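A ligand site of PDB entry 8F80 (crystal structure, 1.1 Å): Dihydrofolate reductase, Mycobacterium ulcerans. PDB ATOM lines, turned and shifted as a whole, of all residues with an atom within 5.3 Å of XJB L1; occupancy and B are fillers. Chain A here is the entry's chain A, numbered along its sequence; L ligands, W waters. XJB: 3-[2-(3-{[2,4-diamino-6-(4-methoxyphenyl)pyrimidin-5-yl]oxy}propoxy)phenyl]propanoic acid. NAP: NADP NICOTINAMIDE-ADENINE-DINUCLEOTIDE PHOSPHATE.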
ATOM      1  N   ILE A  15      13.862  16.247  13.929  1.00  0.00           N
ATOM      2  CA  ILE A  15      13.306  17.146  12.914  1.00  0.00           C
ATOM      3  C   ILE A  15      12.787  18.383  13.611  1.00  0.00           C
ATOM      4  O   ILE A  15      12.067  18.272  14.604  1.00  0.00           O
ATOM      5  CB  ILE A  15      12.231  16.430  12.055  1.00  0.00           C
ATOM      6  CG1 ILE A  15      11.711  17.344  10.939  1.00  0.00           C
ATOM      7  CG2 ILE A  15      11.105  15.861  12.903  1.00  0.00           C
ATOM      8  CD1 ILE A  15      10.975  16.615   9.840  1.00  0.00           C
ATOM      9  N   TRP A  16      13.195  19.559  13.126  1.00  0.00           N
ATOM     10  CA  TRP A  16      12.766  20.817  13.716  1.00  0.00           C
ATOM     11  C   TRP A  16      12.803  21.926  12.668  1.00  0.00           C
ATOM     12  O   TRP A  16      13.470  21.806  11.648  1.00  0.00           O
ATOM     13  CB  TRP A  16      13.594  21.211  14.925  1.00  0.00           C
ATOM     14  CG  TRP A  16      14.970  21.735  14.715  1.00  0.00           C
ATOM     15  CD1 TRP A  16      15.319  23.035  14.482  1.00  0.00           C
ATOM     16  CD2 TRP A  16      16.201  21.017  14.832  1.00  0.00           C
ATOM     17  NE1 TRP A  16      16.673  23.170  14.440  1.00  0.00           N
ATOM     18  CE2 TRP A  16      17.241  21.948  14.651  1.00  0.00           C
ATOM     19  CE3 TRP A  16      16.541  19.681  15.049  1.00  0.00           C
ATOM     20  CZ2 TRP A  16      18.583  21.582  14.694  1.00  0.00           C
ATOM     21  CZ3 TRP A  16      17.868  19.330  15.097  1.00  0.00           C
ATOM     22  CH2 TRP A  16      18.885  20.271  14.913  1.00  0.00           C
ATOM     23  N   ALA A  17      12.091  23.004  12.986  1.00  0.00           N
ATOM     24  CA  ALA A  17      12.144  24.251  12.234  1.00  0.00           C
ATOM     25  C   ALA A  17      12.640  25.362  13.162  1.00  0.00           C
ATOM     26  O   ALA A  17      12.259  25.412  14.333  1.00  0.00           O
ATOM     27  CB  ALA A  17      10.770  24.598  11.684  1.00  0.00           C
ATOM     28  N   ILE A  30       5.002  28.367  18.424  1.00  0.00           N
ATOM     29  CA  ILE A  30       6.054  28.609  17.454  1.00  0.00           C
ATOM     30  C   ILE A  30       5.804  29.974  16.829  1.00  0.00           C
ATOM     31  O   ILE A  30       4.720  30.237  16.332  1.00  0.00           O
ATOM     32  CB  ILE A  30       6.123  27.490  16.393  1.00  0.00           C
ATOM     33  CG1 ILE A  30       6.496  26.170  17.088  1.00  0.00           C
ATOM     34  CG2 ILE A  30       7.121  27.838  15.342  1.00  0.00           C
ATOM     35  CD1 ILE A  30       6.393  24.968  16.246  1.00  0.00           C
ATOM     36  N   ARG A  33       4.545  31.309  11.064  1.00  0.00           N
ATOM     37  CA  ARG A  33       3.692  30.388  10.322  1.00  0.00           C
ATOM     38  C   ARG A  33       4.324  30.135   8.962  1.00  0.00           C
ATOM     39  O   ARG A  33       4.657  31.080   8.235  1.00  0.00           O
ATOM     40  CB  ARG A  33       2.291  30.971  10.174  1.00  0.00           C
ATOM     41  CG  ARG A  33       1.416  30.140   9.276  1.00  0.00           C
ATOM     42  CD  ARG A  33      -0.027  30.577   9.304  1.00  0.00           C
ATOM     43  NE  ARG A  33      -0.827  29.853   8.315  1.00  0.00           N
ATOM     44  CZ  ARG A  33      -1.305  28.620   8.484  1.00  0.00           C
ATOM     45  NH1 ARG A  33      -1.114  27.952   9.608  1.00  0.00           N
ATOM     46  NH2 ARG A  33      -2.000  28.058   7.490  1.00  0.00           N
ATOM     47  N   ASP A  37       6.573  24.333   5.515  1.00  0.00           N
ATOM     48  CA  ASP A  37       7.261  23.501   6.490  1.00  0.00           C
ATOM     49  C   ASP A  37       6.320  22.463   7.097  1.00  0.00           C
ATOM     50  O   ASP A  37       6.732  21.338   7.366  1.00  0.00           O
ATOM     51  CB  ASP A  37       7.892  24.348   7.604  1.00  0.00           C
ATOM     52  CG  ASP A  37       8.491  23.495   8.686  1.00  0.00           C
ATOM     53  OD1 ASP A  37       9.452  22.742   8.382  1.00  0.00           O
ATOM     54  OD2 ASP A  37       7.948  23.526   9.803  1.00  0.00           O
ATOM     55  N   LEU A  38       5.066  22.834   7.343  1.00  0.00           N
ATOM     56  CA  LEU A  38       4.107  21.836   7.823  1.00  0.00           C
ATOM     57  C   LEU A  38       3.996  20.697   6.828  1.00  0.00           C
ATOM     58  O   LEU A  38       3.983  19.515   7.209  1.00  0.00           O
ATOM     59  CB  LEU A  38       2.746  22.504   8.058  1.00  0.00           C
ATOM     60  CG  LEU A  38       1.626  21.525   8.428  1.00  0.00           C
ATOM     61  CD1 LEU A  38       1.962  20.688   9.654  1.00  0.00           C
ATOM     62  CD2 LEU A  38       0.342  22.302   8.644  1.00  0.00           C
ATOM     63  N   HIS A  40       6.241  19.687   4.613  1.00  0.00           N
ATOM     64  CA  HIS A  40       7.488  18.940   4.706  1.00  0.00           C
ATOM     65  C   HIS A  40       7.491  18.017   5.909  1.00  0.00           C
ATOM     66  O   HIS A  40       7.848  16.835   5.805  1.00  0.00           O
ATOM     67  CB  HIS A  40       8.616  19.978   4.807  1.00  0.00           C
ATOM     68  CG  HIS A  40       9.966  19.425   5.098  1.00  0.00           C
ATOM     69  ND1 HIS A  40      10.672  18.684   4.181  1.00  0.00           N
ATOM     70  CD2 HIS A  40      10.770  19.575   6.175  1.00  0.00           C
ATOM     71  CE1 HIS A  40      11.856  18.386   4.687  1.00  0.00           C
ATOM     72  NE2 HIS A  40      11.936  18.908   5.904  1.00  0.00           N
ATOM     73  N   PHE A  41       7.104  18.547   7.068  1.00  0.00           N
ATOM     74  CA  PHE A  41       7.067  17.757   8.293  1.00  0.00           C
ATOM     75  C   PHE A  41       6.134  16.568   8.165  1.00  0.00           C
ATOM     76  O   PHE A  41       6.476  15.444   8.538  1.00  0.00           O
ATOM     77  CB  PHE A  41       6.646  18.683   9.446  1.00  0.00           C
ATOM     78  CG  PHE A  41       6.431  17.942  10.735  1.00  0.00           C
ATOM     79  CD1 PHE A  41       7.511  17.512  11.491  1.00  0.00           C
ATOM     80  CD2 PHE A  41       5.159  17.657  11.201  1.00  0.00           C
ATOM     81  CE1 PHE A  41       7.311  16.793  12.649  1.00  0.00           C
ATOM     82  CE2 PHE A  41       4.960  16.951  12.365  1.00  0.00           C
ATOM     83  CZ  PHE A  41       6.036  16.526  13.091  1.00  0.00           C
ATOM     84  N   LYS A  42       4.952  16.797   7.583  1.00  0.00           N
ATOM     85  CA  LYS A  42       4.020  15.691   7.386  1.00  0.00           C
ATOM     86  C   LYS A  42       4.576  14.649   6.413  1.00  0.00           C
ATOM     87  O   LYS A  42       4.469  13.451   6.663  1.00  0.00           O
ATOM     88  CB  LYS A  42       2.676  16.253   6.922  1.00  0.00           C
ATOM     89  CG  LYS A  42       1.985  17.022   8.028  1.00  0.00           C
ATOM     90  CD  LYS A  42       0.886  17.959   7.536  1.00  0.00           C
ATOM     91  CE  LYS A  42      -0.241  17.215   6.829  1.00  0.00           C
ATOM     92  NZ  LYS A  42      -1.361  18.139   6.466  1.00  0.00           N
ATOM     93  N   THR A  45       7.247  12.516   8.233  1.00  0.00           N
ATOM     94  CA  THR A  45       6.845  11.768   9.408  1.00  0.00           C
ATOM     95  C   THR A  45       5.649  10.846   9.189  1.00  0.00           C
ATOM     96  O   THR A  45       5.416   9.976  10.031  1.00  0.00           O
ATOM     97  CB  THR A  45       6.537  12.684  10.603  1.00  0.00           C
ATOM     98  OG1 THR A  45       5.443  13.565  10.318  1.00  0.00           O
ATOM     99  CG2 THR A  45       7.776  13.470  11.051  1.00  0.00           C
ATOM    100  N   THR A  56       5.304  20.009  24.241  1.00  0.00           N
ATOM    101  CA  THR A  56       4.934  20.045  22.826  1.00  0.00           C
ATOM    102  C   THR A  56       3.586  19.383  22.599  1.00  0.00           C
ATOM    103  O   THR A  56       2.753  19.908  21.861  1.00  0.00           O
ATOM    104  CB  THR A  56       6.053  19.410  21.998  1.00  0.00           C
ATOM    105  OG1 THR A  56       7.192  20.265  22.075  1.00  0.00           O
ATOM    106  CG2 THR A  56       5.676  19.252  20.554  1.00  0.00           C
ATOM    107  N   SER A  59       1.012  21.734  23.461  1.00  0.00           N
ATOM    108  CA  SER A  59       1.015  22.856  22.538  1.00  0.00           C
ATOM    109  C   SER A  59       0.232  22.582  21.272  1.00  0.00           C
ATOM    110  O   SER A  59      -0.092  23.532  20.552  1.00  0.00           O
ATOM    111  CB  SER A  59       2.457  23.249  22.149  1.00  0.00           C
ATOM    112  OG  SER A  59       2.998  22.461  21.082  1.00  0.00           O
ATOM    113  N   LEU A  60      -0.072  21.326  20.993  1.00  0.00           N
ATOM    114  CA  LEU A  60      -0.716  20.991  19.734  1.00  0.00           C
ATOM    115  C   LEU A  60      -2.159  21.486  19.755  1.00  0.00           C
ATOM    116  O   LEU A  60      -2.907  21.188  20.687  1.00  0.00           O
ATOM    117  CB  LEU A  60      -0.715  19.493  19.481  1.00  0.00           C
ATOM    118  CG  LEU A  60       0.669  18.860  19.307  1.00  0.00           C
ATOM    119  CD1 LEU A  60       0.543  17.356  19.242  1.00  0.00           C
ATOM    120  CD2 LEU A  60       1.346  19.369  18.077  1.00  0.00           C
ATOM    121  N   PRO A  61      -2.600  22.202  18.713  1.00  0.00           N
ATOM    122  CA  PRO A  61      -4.024  22.536  18.600  1.00  0.00           C
ATOM    123  C   PRO A  61      -4.834  21.260  18.510  1.00  0.00           C
ATOM    124  O   PRO A  61      -4.351  20.234  18.017  1.00  0.00           O
ATOM    125  CB  PRO A  61      -4.103  23.342  17.303  1.00  0.00           C
ATOM    126  CG  PRO A  61      -2.702  23.802  17.039  1.00  0.00           C
ATOM    127  CD  PRO A  61      -1.817  22.731  17.585  1.00  0.00           C
ATOM    128  N   HIS A  64      -4.881  18.856  15.653  1.00  0.00           N
ATOM    129  CA  HIS A  64      -3.624  18.196  15.326  1.00  0.00           C
ATOM    130  C   HIS A  64      -3.098  17.361  16.488  1.00  0.00           C
ATOM    131  O   HIS A  64      -1.921  17.000  16.495  1.00  0.00           O
ATOM    132  CB  HIS A  64      -2.573  19.256  14.978  1.00  0.00           C
ATOM    133  CG  HIS A  64      -2.953  20.087  13.794  1.00  0.00           C
ATOM    134  ND1 HIS A  64      -2.890  19.609  12.499  1.00  0.00           N
ATOM    135  CD2 HIS A  64      -3.431  21.344  13.704  1.00  0.00           C
ATOM    136  CE1 HIS A  64      -3.313  20.543  11.670  1.00  0.00           C
ATOM    137  NE2 HIS A  64      -3.629  21.616  12.370  1.00  0.00           N
ATOM    138  N   LEU A  67      -1.194  13.853  16.341  1.00  0.00           N
ATOM    139  CA  LEU A  67      -0.820  14.064  14.947  1.00  0.00           C
ATOM    140  C   LEU A  67      -1.355  12.900  14.117  1.00  0.00           C
ATOM    141  O   LEU A  67      -0.962  11.749  14.361  1.00  0.00           O
ATOM    142  CB  LEU A  67       0.701  14.142  14.843  1.00  0.00           C
ATOM    143  CG  LEU A  67       1.266  15.389  15.519  1.00  0.00           C
ATOM    144  CD1 LEU A  67       2.756  15.260  15.664  1.00  0.00           C
ATOM    145  CD2 LEU A  67       0.935  16.643  14.771  1.00  0.00           C
ATOM    146  N   PRO A  68      -2.267  13.129  13.182  1.00  0.00           N
ATOM    147  CA  PRO A  68      -2.928  11.987  12.551  1.00  0.00           C
ATOM    148  C   PRO A  68      -1.984  11.199  11.666  1.00  0.00           C
ATOM    149  O   PRO A  68      -1.092  11.751  11.017  1.00  0.00           O
ATOM    150  CB  PRO A  68      -4.052  12.624  11.728  1.00  0.00           C
ATOM    151  CG  PRO A  68      -3.585  14.004  11.503  1.00  0.00           C
ATOM    152  CD  PRO A  68      -2.863  14.404  12.756  1.00  0.00           C
ATOM    153  N   ARG A  70       0.255   9.056  12.569  1.00  0.00           N
ATOM    154  CA  ARG A  70       1.537   8.809  13.193  1.00  0.00           C
ATOM    155  C   ARG A  70       1.282   8.232  14.558  1.00  0.00           C
ATOM    156  O   ARG A  70       0.253   8.498  15.163  1.00  0.00           O
ATOM    157  CB  ARG A  70       2.303  10.107  13.292  1.00  0.00           C
ATOM    158  CG  ARG A  70       2.868  10.385  11.940  1.00  0.00           C
ATOM    159  CD  ARG A  70       3.000  11.842  11.632  1.00  0.00           C
ATOM    160  NE  ARG A  70       1.722  12.488  11.381  1.00  0.00           N
ATOM    161  CZ  ARG A  70       1.598  13.798  11.183  1.00  0.00           C
ATOM    162  NH1 ARG A  70       2.655  14.589  11.151  1.00  0.00           N
ATOM    163  NH2 ARG A  70       0.387  14.332  11.079  1.00  0.00           N
ATOM    164  N   VAL A 107      12.061  12.302  16.362  1.00  0.00           N
ATOM    165  CA  VAL A 107      11.947  13.129  17.562  1.00  0.00           C
ATOM    166  C   VAL A 107      11.594  14.532  17.092  1.00  0.00           C
ATOM    167  O   VAL A 107      12.336  15.142  16.315  1.00  0.00           O
ATOM    168  CB  VAL A 107      13.251  13.074  18.368  1.00  0.00           C
ATOM    169  CG1 VAL A 107      13.153  14.032  19.529  1.00  0.00           C
ATOM    170  CG2 VAL A 107      13.541  11.653  18.802  1.00  0.00           C
ATOM    171  N   ILE A 108      10.441  15.025  17.525  1.00  0.00           N
ATOM    172  CA  ILE A 108       9.783  16.178  16.920  1.00  0.00           C
ATOM    173  C   ILE A 108       9.717  17.371  17.857  1.00  0.00           C
ATOM    174  O   ILE A 108       9.030  18.349  17.554  1.00  0.00           O
ATOM    175  CB  ILE A 108       8.406  15.827  16.355  1.00  0.00           C
ATOM    176  CG1 ILE A 108       7.403  15.521  17.471  1.00  0.00           C
ATOM    177  CG2 ILE A 108       8.509  14.679  15.356  1.00  0.00           C
ATOM    178  CD1 ILE A 108       5.963  15.566  16.998  1.00  0.00           C
ATOM    179  N   GLY A 109      10.441  17.334  18.979  1.00  0.00           N
ATOM    180  CA  GLY A 109      10.616  18.467  19.862  1.00  0.00           C
ATOM    181  C   GLY A 109       9.951  18.237  21.211  1.00  0.00           C
ATOM    182  O   GLY A 109       9.322  17.210  21.451  1.00  0.00           O
ATOM    183  N   TYR A 114      14.784  17.360  22.429  1.00  0.00           N
ATOM    184  CA  TYR A 114      15.905  17.345  21.492  1.00  0.00           C
ATOM    185  C   TYR A 114      17.216  17.112  22.244  1.00  0.00           C
ATOM    186  O   TYR A 114      18.083  16.373  21.777  1.00  0.00           O
ATOM    187  CB  TYR A 114      16.030  18.634  20.679  1.00  0.00           C
ATOM    188  CG  TYR A 114      14.933  18.871  19.649  1.00  0.00           C
ATOM    189  CD1 TYR A 114      14.490  17.860  18.801  1.00  0.00           C
ATOM    190  CD2 TYR A 114      14.339  20.117  19.534  1.00  0.00           C
ATOM    191  CE1 TYR A 114      13.478  18.083  17.885  1.00  0.00           C
ATOM    192  CE2 TYR A 114      13.339  20.348  18.631  1.00  0.00           C
ATOM    193  CZ  TYR A 114      12.900  19.333  17.813  1.00  0.00           C
ATOM    194  OH  TYR A 114      11.861  19.608  16.958  1.00  0.00           O
ATOM    195  N   GLU A 125      16.934  16.778  10.479  1.00  0.00           N
ATOM    196  CA  GLU A 125      16.258  17.434   9.372  1.00  0.00           C
ATOM    197  C   GLU A 125      15.776  18.796   9.867  1.00  0.00           C
ATOM    198  O   GLU A 125      14.896  18.866  10.736  1.00  0.00           O
ATOM    199  CB  GLU A 125      15.097  16.578   8.873  1.00  0.00           C
ATOM    200  CG  GLU A 125      15.549  15.289   8.223  1.00  0.00           C
ATOM    201  CD  GLU A 125      16.354  15.503   6.940  1.00  0.00           C
ATOM    202  OE1 GLU A 125      16.290  16.621   6.358  1.00  0.00           O
ATOM    203  OE2 GLU A 125      17.050  14.550   6.525  1.00  0.00           O
ATOM    204  N   THR A 127      14.479  22.784   9.114  1.00  0.00           N
ATOM    205  CA  THR A 127      14.003  23.871   8.262  1.00  0.00           C
ATOM    206  C   THR A 127      14.457  25.184   8.875  1.00  0.00           C
ATOM    207  O   THR A 127      14.207  25.435  10.051  1.00  0.00           O
ATOM    208  CB  THR A 127      12.485  23.863   8.157  1.00  0.00           C
ATOM    209  OG1 THR A 127      12.091  22.582   7.678  1.00  0.00           O
ATOM    210  CG2 THR A 127      11.991  24.946   7.205  1.00  0.00           C
HETATM  211  C16 XJB L   1       7.413  21.466  12.730  1.00  0.00           C
HETATM  212  C18 XJB L   1       5.700  22.875  13.882  1.00  0.00           C
HETATM  213  C21 XJB L   1       1.820  24.538  11.677  1.00  0.00           C
HETATM  214  C20 XJB L   1       3.841  23.736  12.683  1.00  0.00           C
HETATM  215  C17 XJB L   1       6.208  22.330  12.715  1.00  0.00           C
HETATM  216  C14 XJB L   1       0.544  18.969  12.375  1.00  0.00           C
HETATM  217  C13 XJB L   1       1.748  19.555  13.057  1.00  0.00           C
HETATM  218  C5  XJB L   1       5.323  19.509  16.279  1.00  0.00           C
HETATM  219  C2  XJB L   1       8.960  19.936  13.661  1.00  0.00           C
HETATM  220  C6  XJB L   1       4.308  20.618  16.265  1.00  0.00           C
HETATM  221  C3  XJB L   1       7.758  20.688  13.791  1.00  0.00           C
HETATM  222  C8  XJB L   1       2.049  22.250  15.769  1.00  0.00           C
HETATM  223  C12 XJB L   1       1.462  20.777  13.930  1.00  0.00           C
HETATM  224  C9  XJB L   1       0.944  23.036  15.498  1.00  0.00           C
HETATM  225  C4  XJB L   1       6.120  19.430  15.001  1.00  0.00           C
HETATM  226  C1  XJB L   1       9.328  20.818  11.586  1.00  0.00           C
HETATM  227  C10 XJB L   1       0.102  22.709  14.466  1.00  0.00           C
HETATM  228  C11 XJB L   1       0.358  21.592  13.698  1.00  0.00           C
HETATM  229  C15 XJB L   1       0.797  17.697  11.593  1.00  0.00           C
HETATM  230  C19 XJB L   1       4.542  23.625  13.857  1.00  0.00           C
HETATM  231  C22 XJB L   1       4.269  23.104  11.539  1.00  0.00           C
HETATM  232  C23 XJB L   1       5.430  22.378  11.561  1.00  0.00           C
HETATM  233  C7  XJB L   1       2.300  21.129  14.995  1.00  0.00           C
HETATM  234  N1  XJB L   1      10.062  20.893  10.470  1.00  0.00           N
HETATM  235  N2  XJB L   1       9.732  20.003  12.576  1.00  0.00           N
HETATM  236  N3  XJB L   1       9.357  19.121  14.672  1.00  0.00           N
HETATM  237  N4  XJB L   1       8.212  21.570  11.641  1.00  0.00           N
HETATM  238  O1  XJB L   1       6.990  20.572  14.918  1.00  0.00           O
HETATM  239  O2  XJB L   1       3.381  20.311  15.220  1.00  0.00           O
HETATM  240  O3  XJB L   1       1.963  17.299  11.412  1.00  0.00           O
HETATM  241  O4  XJB L   1      -0.197  17.084  11.159  1.00  0.00           O
HETATM  242  O5  XJB L   1       2.705  24.484  12.787  1.00  0.00           O
HETATM  243  PA  NAP L   2       9.361  19.812  25.545  1.00  0.00           P
HETATM  244  O1A NAP L   2      10.738  19.291  25.305  1.00  0.00           O
HETATM  245  O2A NAP L   2       8.361  19.723  24.451  1.00  0.00           O
HETATM  246  O5B NAP L   2       8.669  19.112  26.795  1.00  0.00           O
HETATM  247  C5B NAP L   2       9.253  19.178  28.103  1.00  0.00           C
HETATM  248  C4B NAP L   2       8.605  18.139  28.973  1.00  0.00           C
HETATM  249  O4B NAP L   2       9.088  16.828  28.578  1.00  0.00           O
HETATM  250  C3B NAP L   2       8.914  18.234  30.474  1.00  0.00           C
HETATM  251  O3B NAP L   2       8.139  19.255  31.076  1.00  0.00           O
HETATM  252  C2B NAP L   2       8.589  16.813  30.882  1.00  0.00           C
HETATM  253  O2B NAP L   2       7.195  16.543  30.870  1.00  0.00           O
HETATM  254  C1B NAP L   2       9.187  16.018  29.712  1.00  0.00           C
HETATM  255  N9A NAP L   2      10.577  15.651  29.950  1.00  0.00           N
HETATM  256  C8A NAP L   2      11.709  16.399  29.749  1.00  0.00           C
HETATM  257  N7A NAP L   2      12.804  15.768  30.076  1.00  0.00           N
HETATM  258  C5A NAP L   2      12.368  14.536  30.532  1.00  0.00           C
HETATM  259  C6A NAP L   2      13.052  13.400  31.014  1.00  0.00           C
HETATM  260  N6A NAP L   2      14.377  13.351  31.148  1.00  0.00           N
HETATM  261  N1A NAP L   2      12.314  12.329  31.363  1.00  0.00           N
HETATM  262  C2A NAP L   2      10.979  12.398  31.241  1.00  0.00           C
HETATM  263  N3A NAP L   2      10.221  13.409  30.816  1.00  0.00           N
HETATM  264  C4A NAP L   2      10.992  14.449  30.444  1.00  0.00           C
HETATM  265  O3  NAP L   2       9.420  21.325  26.106  1.00  0.00           O
HETATM  266  PN  NAP L   2      10.227  22.634  25.705  1.00  0.00           P
HETATM  267  O1N NAP L   2      11.692  22.364  25.711  1.00  0.00           O
HETATM  268  O2N NAP L   2       9.700  23.719  26.566  1.00  0.00           O
HETATM  269  O5D NAP L   2       9.820  22.862  24.183  1.00  0.00           O
HETATM  270  C5D NAP L   2       8.495  23.311  23.879  1.00  0.00           C
HETATM  271  C4D NAP L   2       8.579  24.458  22.898  1.00  0.00           C
HETATM  272  O4D NAP L   2       9.144  24.024  21.654  1.00  0.00           O
HETATM  273  C3D NAP L   2       7.215  25.062  22.542  1.00  0.00           C
HETATM  274  O3D NAP L   2       7.364  26.463  22.329  1.00  0.00           O
HETATM  275  C2D NAP L   2       6.871  24.354  21.234  1.00  0.00           C
HETATM  276  O2D NAP L   2       5.964  25.084  20.443  1.00  0.00           O
HETATM  277  C1D NAP L   2       8.257  24.363  20.597  1.00  0.00           C
HETATM  278  N1N NAP L   2       8.460  23.395  19.513  1.00  0.00           N
HETATM  279  C2N NAP L   2       9.033  23.848  18.351  1.00  0.00           C
HETATM  280  C3N NAP L   2       9.281  22.948  17.316  1.00  0.00           C
HETATM  281  C7N NAP L   2       9.917  23.442  16.057  1.00  0.00           C
HETATM  282  O7N NAP L   2      10.290  22.622  15.217  1.00  0.00           O
HETATM  283  N7N NAP L   2      10.038  24.749  15.857  1.00  0.00           N
HETATM  284  C4N NAP L   2       8.973  21.614  17.491  1.00  0.00           C
HETATM  285  C5N NAP L   2       8.413  21.184  18.672  1.00  0.00           C
HETATM  286  C6N NAP L   2       8.159  22.077  19.686  1.00  0.00           C
HETATM  287  P2B NAP L   2       6.335  16.626  32.244  1.00  0.00           P
HETATM  288  O1X NAP L   2       4.960  16.205  31.811  1.00  0.00           O
HETATM  289  O2X NAP L   2       6.986  15.668  33.214  1.00  0.00           O
HETATM  290  O3X NAP L   2       6.411  18.071  32.687  1.00  0.00           O
HETATM  291  O   HOH W   1       3.287  27.885  12.788  1.00  0.00           O
HETATM  292  O   HOH W   2      -2.664  17.392  11.542  1.00  0.00           O
HETATM  293  O   HOH W   3       2.328  26.383  15.205  1.00  0.00           O
HETATM  294  O   HOH W   4      12.564  20.083   9.023  1.00  0.00           O
HETATM  295  O   HOH W   5       1.308  26.188   8.821  1.00  0.00           O
HETATM  296  O   HOH W   6       4.112  26.714  10.394  1.00  0.00           O
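Trp 16 touches XJB L1.
Ala 17 touches XJB L1 (N to C1, 3.8 Å).
CD1 of Ile 30 touches C18 of XJB L1 (3.2 Å).
Leu 38 touches XJB L1 (CD1 to C14, 3.5 Å).
CE2 of Phe 41 touches O3 of XJB L1, at 3.2 Å.
Lys 42 touches XJB L1 (CG to O3, 3.4 Å).
CD2 of Leu 60 touches O2 of XJB L1, at 3.6 Å.
CD of Pro 61 touches C9 of XJB L1, at 3.5 Å.
ND1 of His 64 touches C14 of XJB L1 (3.5 Å).
CD2 of Leu 67 touches C15 of XJB L1, 3.4 Å away.
OG1 of Thr 127 touches N1 of XJB L1, 3.8 Å away.
OD2 of Asp 37 sits at hydrogen-bond distance from N4 of XJB L1.
An oxygen (O3) of XJB L1 lies within salt-bridge range of the guanidinium group of Arg 70 (2.8 Å).
O of Ile 15 is in hydrogen-bond range of N3 of XJB L1, 2.8 Å away.
A nitrogen (N3) of XJB L1 lies within hydrogen-bond range of the backbone carbonyl oxygen (O) of Ile 108, 3.0 Å away.
A nitrogen (N3) of XJB L1 is in hydrogen-bond range of the side-chain hydroxyl of Tyr 114.
O7N of NAP L2 lies within hydrogen-bond range of N of Ala 17, 2.9 Å away.
The backbone carbonyl oxygen (O) of Ala 17 sits at hydrogen-bond distance from a nitrogen (N7N) of NAP L2 (2.8 Å).
The backbone NH (N) of Thr 56 is in hydrogen-bond range of an oxygen (O2A) of NAP L2, 3.1 Å away.
An oxygen (O2A) of NAP L2 sits at hydrogen-bond distance from the side-chain hydroxyl of Thr 56 (2.7 Å).
Water W2 bridges a ring nitrogen (ND1) of His 64 (2.4 Å) and an oxygen (O4) of XJB L1 (2.5 Å).
Water W4 lies within hydrogen-bond range of OG1 of Thr 127 (2.9 Å), N1 of XJB L1 (3.0 Å), O of Glu 125 (3.1 Å), O of Trp 16 (3.3 Å) and NE2 of His 40 (3.4 Å).
OG1 of Thr 127 sits at hydrogen-bond distance from OD1 of Asp 37 (2.7 Å).
The backbone carbonyl oxygen (O) of Ile 15 sits at hydrogen-bond distance from the side-chain hydroxyl (OH) of Tyr 114, at 2.7 Å.
N of Ile 15 lies within hydrogen-bond range of O of Val 107.
The side-chain hydroxyl of Tyr 114 is in hydrogen-bond range of the backbone carbonyl oxygen of Ile 108 (3.2 Å).
O of Phe 41 sits at hydrogen-bond distance from OG1 of Thr 45 (2.8 Å).
The backbone carbonyl oxygen of Trp 16 lies within hydrogen-bond range of the backbone NH of Thr 127 (2.9 Å).
The backbone carbonyl oxygen (O) of Glu 125 lies within hydrogen-bond range of the backbone NH (N) of Trp 16.
N of Gly 109 lies close to OH of Tyr 114 (3.4 Å).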
